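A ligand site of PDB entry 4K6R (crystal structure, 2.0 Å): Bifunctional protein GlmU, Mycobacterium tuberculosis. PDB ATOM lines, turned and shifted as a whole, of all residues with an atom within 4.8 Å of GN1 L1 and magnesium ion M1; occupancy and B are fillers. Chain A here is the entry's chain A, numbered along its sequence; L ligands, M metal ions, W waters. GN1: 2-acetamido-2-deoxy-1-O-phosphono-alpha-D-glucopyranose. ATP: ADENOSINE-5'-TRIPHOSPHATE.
OE2 of Glu 172 sits at hydrogen-bond distance from O3 of GN1 L1, at 2.7 Å.
An oxygen (O4) of GN1 L1 is in hydrogen-bond range of the backbone NH (N) of Gly 157.
O2G of ATP L2 sits at hydrogen-bond distance from N of Arg 25 (3.0 Å).
NE of Arg 25 is in salt-bridge range of O2G of ATP L2 (2.8 Å).
The backbone carbonyl oxygen (O) of Asn 187 lies within hydrogen-bond range of an oxygen (O4) of GN1 L1.
An oxygen (O3) of GN1 L1 sits at hydrogen-bond distance from the side-chain amide nitrogen (ND2) of Asn 187 (2.8 Å).
An oxygen (OP3) of GN1 L1 lies within salt-bridge range of the guanidinium group (NH2) of Arg 25.
The side-chain hydroxyl (OG1) of Thr 95 lies within hydrogen-bond range of an oxygen (O7) of GN1 L1.
OH of Tyr 156 lies within hydrogen-bond range of N of Gly 243, at 3.0 Å.
The side-chain amide nitrogen (ND2) of Asn 245 lies close to the guanidinium group (NH2) of Arg 25, 3.3 Å away.
OD1 of Asn 245 lies close to NZ of Lys 32 (3.0 Å).
N of Asn 187 sits at hydrogen-bond distance from O of Gly 157 (2.8 Å).
The side-chain carboxylate (OD2) of Asp 120 lies close to the side-chain amino group (NZ) of Lys 32 (2.9 Å).
O of Asp 120 is in hydrogen-bond range of N of Val 244.
The side-chain hydroxyl (OH) of Tyr 191 lies within hydrogen-bond range of the side-chain amide nitrogen (ND2) of Asn 187.
The backbone NH (N) of Gly 189 lies within hydrogen-bond range of the side-chain amide oxygen (OD1) of Asn 187, 3.0 Å away.
Merely in contact with GN1 L1: Tyr 156, Ala 188, Tyr 215, Thr 217 and Gly 243.
Of the 20 residues printed, 11 come within 4 Å of GN1 L1.
The nearest printed residue that does not touch GN1 L1 is Asp 120 (4.1 Å).
Merely in contact with magnesium ion M1: Lys 32 (3.8 Å).
Three residues have an atom within 4 Å of magnesium ion M1: Lys 32, Asp 120 and Asn 245.
The nearest printed residue that does not touch magnesium ion M1 is Val 244 (4.3 Å).
Magnesium ion M1 is bound by OD2 of Asp 120, at 2.0 Å.
Magnesium ion M1 is bound by OP2 of GN1 L1, at 2.0 Å.
The side-chain amide oxygen (OD1) of Asn 245 is bound to magnesium ion M1 (2.1 Å).
Water W4 binds magnesium ion M1 (2.2 Å).
Magnesium ion M1 is bound by water W10, at 2.2 Å.
Water W6 is bound to magnesium ion M1 (2.2 Å).
Water W6 lies within hydrogen-bond range of O2B of ATP L2 (2.6 Å), NZ of Lys 32 (3.2 Å) and OP1 of GN1 L1 (3.5 Å).
Water W4 lies within hydrogen-bond range of the side-chain carboxylate (OD1) of Asp 120 (2.6 Å) and an oxygen (O5) of GN1 L1 (3.0 Å).
Water W8 lies within hydrogen-bond range of an oxygen (OP3) of GN1 L1 (2.6 Å), the backbone carbonyl oxygen (O) of Gly 155 (2.9 Å), the guanidinium group (NH1) of Arg 25 (3.1 Å) and the side-chain amide nitrogen (ND2) of Asn 245 (3.2 Å).
Water W11 bridges the side-chain hydroxyl (OH) of Tyr 191 (2.6 Å) and an oxygen (O7) of GN1 L1 (2.6 Å).
Water W9 lies within hydrogen-bond range of an oxygen (O6) of GN1 L1 (2.7 Å), the backbone carbonyl oxygen (O) of Ala 188 (2.7 Å), the side-chain hydroxyl (OG1) of Thr 121 (3.1 Å) and the backbone NH (N) of Gly 243 (3.4 Å).
Water W5 lies within hydrogen-bond range of OP3 of GN1 L1 (2.8 Å), O2B of ATP L2 (2.9 Å) and NH2 of Arg 25 (3.2 Å).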
ATOM      1  N   ARG A  25     -15.324 -22.760  22.328  1.00  0.00           N
ATOM      2  CA  ARG A  25     -16.516 -21.853  22.434  1.00  0.00           C
ATOM      3  C   ARG A  25     -17.657 -22.192  21.457  1.00  0.00           C
ATOM      4  O   ARG A  25     -18.792 -21.820  21.712  1.00  0.00           O
ATOM      5  CB  ARG A  25     -16.120 -20.374  22.313  1.00  0.00           C
ATOM      6  CG  ARG A  25     -15.454 -19.919  23.632  1.00  0.00           C
ATOM      7  CD  ARG A  25     -14.827 -18.541  23.415  1.00  0.00           C
ATOM      8  NE  ARG A  25     -13.729 -18.641  22.416  1.00  0.00           N
ATOM      9  CZ  ARG A  25     -13.022 -17.566  22.000  1.00  0.00           C
ATOM     10  NH1 ARG A  25     -13.371 -16.320  22.400  1.00  0.00           N
ATOM     11  NH2 ARG A  25     -11.985 -17.691  21.158  1.00  0.00           N
ATOM     12  N   LYS A  32     -14.418 -26.447  14.179  1.00  0.00           N
ATOM     13  CA  LYS A  32     -14.962 -25.109  13.975  1.00  0.00           C
ATOM     14  C   LYS A  32     -14.839 -24.569  12.574  1.00  0.00           C
ATOM     15  O   LYS A  32     -15.832 -24.016  12.044  1.00  0.00           O
ATOM     16  CB  LYS A  32     -14.243 -24.127  14.929  1.00  0.00           C
ATOM     17  CG  LYS A  32     -14.590 -22.640  14.698  1.00  0.00           C
ATOM     18  CD  LYS A  32     -13.941 -21.829  15.854  1.00  0.00           C
ATOM     19  CE  LYS A  32     -13.701 -20.447  15.465  1.00  0.00           C
ATOM     20  NZ  LYS A  32     -12.823 -19.716  16.504  1.00  0.00           N
ATOM     21  N   THR A  95      -1.684 -17.900  18.879  1.00  0.00           N
ATOM     22  CA  THR A  95      -1.539 -17.478  17.463  1.00  0.00           C
ATOM     23  C   THR A  95      -0.108 -17.120  17.052  1.00  0.00           C
ATOM     24  O   THR A  95       0.220 -17.215  15.866  1.00  0.00           O
ATOM     25  CB  THR A  95      -2.421 -16.272  17.171  1.00  0.00           C
ATOM     26  OG1 THR A  95      -2.174 -15.259  18.172  1.00  0.00           O
ATOM     27  CG2 THR A  95      -3.970 -16.746  17.273  1.00  0.00           C
ATOM     28  N   ASP A 120     -11.084 -18.155  10.803  1.00  0.00           N
ATOM     29  CA  ASP A 120     -12.481 -17.865  11.295  1.00  0.00           C
ATOM     30  C   ASP A 120     -12.902 -16.455  10.967  1.00  0.00           C
ATOM     31  O   ASP A 120     -13.785 -15.876  11.667  1.00  0.00           O
ATOM     32  CB  ASP A 120     -12.679 -18.171  12.811  1.00  0.00           C
ATOM     33  CG  ASP A 120     -11.720 -17.341  13.754  1.00  0.00           C
ATOM     34  OD1 ASP A 120     -10.929 -16.522  13.268  1.00  0.00           O
ATOM     35  OD2 ASP A 120     -11.793 -17.433  14.999  1.00  0.00           O
ATOM     36  N   THR A 121     -12.323 -15.916   9.879  1.00  0.00           N
ATOM     37  CA  THR A 121     -12.706 -14.593   9.338  1.00  0.00           C
ATOM     38  C   THR A 121     -13.341 -14.831   7.948  1.00  0.00           C
ATOM     39  O   THR A 121     -12.727 -14.597   6.928  1.00  0.00           O
ATOM     40  CB  THR A 121     -11.459 -13.707   9.304  1.00  0.00           C
ATOM     41  OG1 THR A 121     -10.922 -13.675  10.615  1.00  0.00           O
ATOM     42  CG2 THR A 121     -11.788 -12.227   8.971  1.00  0.00           C
ATOM     43  N   GLY A 155     -14.588  -9.608  22.900  1.00  0.00           N
ATOM     44  CA  GLY A 155     -13.728 -10.726  22.456  1.00  0.00           C
ATOM     45  C   GLY A 155     -12.696 -10.390  21.381  1.00  0.00           C
ATOM     46  O   GLY A 155     -11.840 -11.251  21.042  1.00  0.00           O
ATOM     47  N   TYR A 156     -12.701  -9.156  20.864  1.00  0.00           N
ATOM     48  CA  TYR A 156     -11.672  -8.737  19.897  1.00  0.00           C
ATOM     49  C   TYR A 156     -10.496  -8.110  20.649  1.00  0.00           C
ATOM     50  O   TYR A 156     -10.712  -7.606  21.747  1.00  0.00           O
ATOM     51  CB  TYR A 156     -12.212  -7.624  18.963  1.00  0.00           C
ATOM     52  CG  TYR A 156     -13.130  -8.101  17.871  1.00  0.00           C
ATOM     53  CD1 TYR A 156     -12.621  -8.410  16.607  1.00  0.00           C
ATOM     54  CD2 TYR A 156     -14.508  -8.248  18.099  1.00  0.00           C
ATOM     55  CE1 TYR A 156     -13.435  -8.832  15.589  1.00  0.00           C
ATOM     56  CE2 TYR A 156     -15.346  -8.710  17.066  1.00  0.00           C
ATOM     57  CZ  TYR A 156     -14.776  -8.978  15.823  1.00  0.00           C
ATOM     58  OH  TYR A 156     -15.581  -9.449  14.825  1.00  0.00           O
ATOM     59  N   GLY A 157      -9.288  -8.147  20.047  1.00  0.00           N
ATOM     60  CA  GLY A 157      -8.174  -7.331  20.530  1.00  0.00           C
ATOM     61  C   GLY A 157      -8.585  -5.863  20.258  1.00  0.00           C
ATOM     62  O   GLY A 157      -9.147  -5.567  19.185  1.00  0.00           O
ATOM     63  N   ILE A 170      -1.838  -3.909  20.630  1.00  0.00           N
ATOM     64  CA  ILE A 170      -3.157  -4.542  20.595  1.00  0.00           C
ATOM     65  C   ILE A 170      -3.291  -5.249  21.970  1.00  0.00           C
ATOM     66  O   ILE A 170      -2.360  -5.972  22.398  1.00  0.00           O
ATOM     67  CB  ILE A 170      -3.241  -5.574  19.422  1.00  0.00           C
ATOM     68  CG1 ILE A 170      -3.009  -4.876  18.078  1.00  0.00           C
ATOM     69  CG2 ILE A 170      -4.627  -6.289  19.513  1.00  0.00           C
ATOM     70  CD1 ILE A 170      -2.931  -5.795  16.869  1.00  0.00           C
ATOM     71  N   GLU A 172      -5.730  -7.802  24.292  1.00  0.00           N
ATOM     72  CA  GLU A 172      -6.800  -8.776  24.085  1.00  0.00           C
ATOM     73  C   GLU A 172      -7.888  -8.573  25.090  1.00  0.00           C
ATOM     74  O   GLU A 172      -7.621  -8.042  26.197  1.00  0.00           O
ATOM     75  CB  GLU A 172      -6.243 -10.188  24.176  1.00  0.00           C
ATOM     76  CG  GLU A 172      -5.290 -10.486  22.990  1.00  0.00           C
ATOM     77  CD  GLU A 172      -6.021 -10.479  21.686  1.00  0.00           C
ATOM     78  OE1 GLU A 172      -6.902 -11.397  21.427  1.00  0.00           O
ATOM     79  OE2 GLU A 172      -5.711  -9.562  20.898  1.00  0.00           O
ATOM     80  N   ASN A 187      -8.874  -5.232  16.395  1.00  0.00           N
ATOM     81  CA  ASN A 187      -7.989  -5.994  15.531  1.00  0.00           C
ATOM     82  C   ASN A 187      -8.750  -7.009  14.665  1.00  0.00           C
ATOM     83  O   ASN A 187      -9.425  -7.878  15.197  1.00  0.00           O
ATOM     84  CB  ASN A 187      -7.010  -6.770  16.436  1.00  0.00           C
ATOM     85  CG  ASN A 187      -5.957  -7.549  15.645  1.00  0.00           C
ATOM     86  OD1 ASN A 187      -5.597  -7.163  14.529  1.00  0.00           O
ATOM     87  ND2 ASN A 187      -5.519  -8.724  16.195  1.00  0.00           N
ATOM     88  N   ALA A 188      -8.534  -6.957  13.335  1.00  0.00           N
ATOM     89  CA  ALA A 188      -9.079  -7.918  12.373  1.00  0.00           C
ATOM     90  C   ALA A 188      -8.381  -9.300  12.487  1.00  0.00           C
ATOM     91  O   ALA A 188      -8.906 -10.329  12.053  1.00  0.00           O
ATOM     92  CB  ALA A 188      -8.851  -7.384  10.953  1.00  0.00           C
ATOM     93  N   GLY A 189      -7.172  -9.275  13.027  1.00  0.00           N
ATOM     94  CA  GLY A 189      -6.267 -10.466  12.958  1.00  0.00           C
ATOM     95  C   GLY A 189      -5.852 -10.782  11.541  1.00  0.00           C
ATOM     96  O   GLY A 189      -5.674 -11.978  11.181  1.00  0.00           O
ATOM     97  N   TYR A 191      -2.907  -9.406   8.777  1.00  0.00           N
ATOM     98  CA  TYR A 191      -1.691  -8.564   8.845  1.00  0.00           C
ATOM     99  C   TYR A 191      -0.837  -8.824   7.620  1.00  0.00           C
ATOM    100  O   TYR A 191      -0.907  -9.898   7.010  1.00  0.00           O
ATOM    101  CB  TYR A 191      -0.785  -9.058   9.993  1.00  0.00           C
ATOM    102  CG  TYR A 191      -1.446  -9.333  11.351  1.00  0.00           C
ATOM    103  CD1 TYR A 191      -2.134 -10.565  11.603  1.00  0.00           C
ATOM    104  CD2 TYR A 191      -1.354  -8.403  12.394  1.00  0.00           C
ATOM    105  CE1 TYR A 191      -2.712 -10.813  12.890  1.00  0.00           C
ATOM    106  CE2 TYR A 191      -1.922  -8.670  13.651  1.00  0.00           C
ATOM    107  CZ  TYR A 191      -2.560  -9.899  13.881  1.00  0.00           C
ATOM    108  OH  TYR A 191      -3.085 -10.100  15.154  1.00  0.00           O
ATOM    109  N   TYR A 215       0.805 -14.564  22.156  1.00  0.00           N
ATOM    110  CA  TYR A 215      -0.208 -13.863  21.370  1.00  0.00           C
ATOM    111  C   TYR A 215       0.504 -13.270  20.095  1.00  0.00           C
ATOM    112  O   TYR A 215       1.427 -12.506  20.244  1.00  0.00           O
ATOM    113  CB  TYR A 215      -0.709 -12.661  22.215  1.00  0.00           C
ATOM    114  CG  TYR A 215      -1.749 -12.906  23.320  1.00  0.00           C
ATOM    115  CD1 TYR A 215      -2.448 -14.100  23.428  1.00  0.00           C
ATOM    116  CD2 TYR A 215      -2.048 -11.879  24.211  1.00  0.00           C
ATOM    117  CE1 TYR A 215      -3.463 -14.272  24.431  1.00  0.00           C
ATOM    118  CE2 TYR A 215      -3.069 -12.015  25.195  1.00  0.00           C
ATOM    119  CZ  TYR A 215      -3.764 -13.260  25.299  1.00  0.00           C
ATOM    120  OH  TYR A 215      -4.768 -13.392  26.245  1.00  0.00           O
ATOM    121  N   LEU A 216       0.024 -13.503  18.896  1.00  0.00           N
ATOM    122  CA  LEU A 216       0.625 -12.834  17.724  1.00  0.00           C
ATOM    123  C   LEU A 216       0.476 -11.324  17.892  1.00  0.00           C
ATOM    124  O   LEU A 216       1.324 -10.550  17.403  1.00  0.00           O
ATOM    125  CB  LEU A 216      -0.105 -13.289  16.442  1.00  0.00           C
ATOM    126  CG  LEU A 216       0.319 -12.638  15.079  1.00  0.00           C
ATOM    127  CD1 LEU A 216       1.821 -12.934  14.787  1.00  0.00           C
ATOM    128  CD2 LEU A 216      -0.568 -13.267  13.949  1.00  0.00           C
ATOM    129  N   THR A 217      -0.597 -10.884  18.546  1.00  0.00           N
ATOM    130  CA  THR A 217      -0.870  -9.463  18.660  1.00  0.00           C
ATOM    131  C   THR A 217       0.210  -8.668  19.411  1.00  0.00           C
ATOM    132  O   THR A 217       0.360  -7.447  19.194  1.00  0.00           O
ATOM    133  CB  THR A 217      -2.182  -9.233  19.370  1.00  0.00           C
ATOM    134  OG1 THR A 217      -2.207 -10.022  20.563  1.00  0.00           O
ATOM    135  CG2 THR A 217      -3.366  -9.648  18.463  1.00  0.00           C
ATOM    136  N   GLY A 243     -14.764 -11.665  12.998  1.00  0.00           N
ATOM    137  CA  GLY A 243     -14.466 -13.063  13.295  1.00  0.00           C
ATOM    138  C   GLY A 243     -15.606 -13.836  13.918  1.00  0.00           C
ATOM    139  O   GLY A 243     -16.613 -13.219  14.391  1.00  0.00           O
ATOM    140  N   VAL A 244     -15.412 -15.162  13.967  1.00  0.00           N
ATOM    141  CA  VAL A 244     -16.403 -16.075  14.497  1.00  0.00           C
ATOM    142  C   VAL A 244     -15.735 -16.926  15.541  1.00  0.00           C
ATOM    143  O   VAL A 244     -14.900 -17.834  15.199  1.00  0.00           O
ATOM    144  CB  VAL A 244     -16.964 -16.962  13.371  1.00  0.00           C
ATOM    145  CG1 VAL A 244     -17.881 -18.155  13.911  1.00  0.00           C
ATOM    146  CG2 VAL A 244     -17.762 -16.144  12.299  1.00  0.00           C
ATOM    147  N   ASN A 245     -16.103 -16.740  16.808  1.00  0.00           N
ATOM    148  CA  ASN A 245     -15.608 -17.641  17.835  1.00  0.00           C
ATOM    149  C   ASN A 245     -16.660 -18.490  18.488  1.00  0.00           C
ATOM    150  O   ASN A 245     -16.355 -19.324  19.350  1.00  0.00           O
ATOM    151  CB  ASN A 245     -14.894 -16.837  18.942  1.00  0.00           C
ATOM    152  CG  ASN A 245     -13.479 -16.375  18.536  1.00  0.00           C
ATOM    153  OD1 ASN A 245     -12.838 -16.918  17.612  1.00  0.00           O
ATOM    154  ND2 ASN A 245     -13.025 -15.317  19.195  1.00  0.00           N
HETATM  155  C1  GN1 L   1      -7.771 -13.269  17.504  1.00  0.00           C
HETATM  156  OP1 GN1 L   1      -7.904 -15.900  18.706  1.00  0.00           O
HETATM  157  P   GN1 L   1      -9.100 -15.044  19.046  1.00  0.00           P
HETATM  158  OP2 GN1 L   1     -10.305 -15.378  18.184  1.00  0.00           O
HETATM  159  OP3 GN1 L   1      -9.374 -14.996  20.526  1.00  0.00           O
HETATM  160  C2  GN1 L   1      -6.814 -12.105  17.837  1.00  0.00           C
HETATM  161  C3  GN1 L   1      -7.644 -10.863  18.199  1.00  0.00           C
HETATM  162  C4  GN1 L   1      -8.552 -10.520  16.999  1.00  0.00           C
HETATM  163  C5  GN1 L   1      -9.421 -11.737  16.633  1.00  0.00           C
HETATM  164  C6  GN1 L   1     -10.121 -11.434  15.312  1.00  0.00           C
HETATM  165  C8  GN1 L   1      -4.017 -13.162  20.310  1.00  0.00           C
HETATM  166  O1  GN1 L   1      -8.573 -13.602  18.627  1.00  0.00           O
HETATM  167  O3  GN1 L   1      -6.750  -9.761  18.442  1.00  0.00           O
HETATM  168  O4  GN1 L   1      -9.366  -9.376  17.368  1.00  0.00           O
HETATM  169  O5  GN1 L   1      -8.607 -12.913  16.415  1.00  0.00           O
HETATM  170  N2  GN1 L   1      -5.990 -12.430  19.057  1.00  0.00           N
HETATM  171  C7  GN1 L   1      -4.770 -12.949  18.987  1.00  0.00           C
HETATM  172  O6  GN1 L   1     -11.023 -12.454  14.899  1.00  0.00           O
HETATM  173  O7  GN1 L   1      -4.287 -13.298  17.928  1.00  0.00           O
HETATM  174  PG  ATP L   2     -11.551 -21.547  22.048  1.00  0.00           P
HETATM  175  O1G ATP L   2     -11.046 -22.927  21.657  1.00  0.00           O
HETATM  176  O2G ATP L   2     -12.938 -21.192  21.562  1.00  0.00           O
HETATM  177  O3G ATP L   2     -11.202 -21.013  23.401  1.00  0.00           O
HETATM  178  PB  ATP L   2      -9.692 -20.735  19.856  1.00  0.00           P
HETATM  179  O1B ATP L   2     -10.208 -21.689  18.864  1.00  0.00           O
HETATM  180  O2B ATP L   2      -9.288 -19.368  19.373  1.00  0.00           O
HETATM  181  O3B ATP L   2     -10.644 -20.526  21.142  1.00  0.00           O
HETATM  182  PA  ATP L   2      -7.510 -21.191  21.818  1.00  0.00           P
HETATM  183  O1A ATP L   2      -7.920 -19.816  22.361  1.00  0.00           O
HETATM  184  O2A ATP L   2      -7.655 -22.428  22.675  1.00  0.00           O
HETATM  185  O3A ATP L   2      -8.349 -21.456  20.434  1.00  0.00           O
HETATM  186  O5' ATP L   2      -6.028 -21.186  21.223  1.00  0.00           O
HETATM  187  C5' ATP L   2      -5.367 -20.018  20.732  1.00  0.00           C
HETATM  188  C4' ATP L   2      -4.392 -20.518  19.686  1.00  0.00           C
HETATM  189  O4' ATP L   2      -3.438 -21.478  20.282  1.00  0.00           O
HETATM  190  C3' ATP L   2      -5.160 -21.297  18.602  1.00  0.00           C
HETATM  191  O3' ATP L   2      -5.516 -20.431  17.512  1.00  0.00           O
HETATM  192  C2' ATP L   2      -4.045 -22.260  18.125  1.00  0.00           C
HETATM  193  O2' ATP L   2      -3.153 -21.561  17.250  1.00  0.00           O
HETATM  194  C1' ATP L   2      -3.255 -22.557  19.388  1.00  0.00           C
HETATM  195  N9  ATP L   2      -3.883 -23.778  19.932  1.00  0.00           N
HETATM  196  C8  ATP L   2      -4.722 -23.785  21.000  1.00  0.00           C
HETATM  197  N7  ATP L   2      -5.039 -25.092  21.253  1.00  0.00           N
HETATM  198  C5  ATP L   2      -4.464 -25.874  20.348  1.00  0.00           C
HETATM  199  C6  ATP L   2      -4.404 -27.314  20.138  1.00  0.00           C
HETATM  200  N6  ATP L   2      -5.139 -28.209  20.893  1.00  0.00           N
HETATM  201  N1  ATP L   2      -3.643 -27.686  19.122  1.00  0.00           N
HETATM  202  C2  ATP L   2      -2.919 -26.865  18.320  1.00  0.00           C
HETATM  203  N3  ATP L   2      -2.901 -25.543  18.463  1.00  0.00           N
HETATM  204  C4  ATP L   2      -3.686 -25.017  19.464  1.00  0.00           C
HETATM  205 MG    MG M   1     -11.120 -16.296  16.546  1.00  0.00          MG
HETATM  206 MG    MG M   2      -8.117 -18.223  23.377  1.00  0.00          MG
HETATM  207  O   HOH W   1      -7.275 -13.939  22.005  1.00  0.00           O
HETATM  208  O   HOH W   2      -7.023 -18.419  18.138  1.00  0.00           O
HETATM  209  O   HOH W   3      -5.898 -15.841  20.596  1.00  0.00           O
HETATM  210  O   HOH W   4      -9.572 -15.472  15.251  1.00  0.00           O
HETATM  211  O   HOH W   5      -8.856 -17.482  21.584  1.00  0.00           O
HETATM  212  O   HOH W   6     -10.140 -18.135  17.247  1.00  0.00           O
HETATM  213  O   HOH W   7      -7.246 -16.651  15.970  1.00  0.00           O
HETATM  214  O   HOH W   8     -11.449 -14.018  21.658  1.00  0.00           O
HETATM  215  O   HOH W   9     -11.449 -11.291  12.448  1.00  0.00           O
HETATM  216  O   HOH W  10     -12.405 -14.585  16.111  1.00  0.00           O
HETATM  217  O   HOH W  11      -4.066 -12.428  15.520  1.00  0.00           O
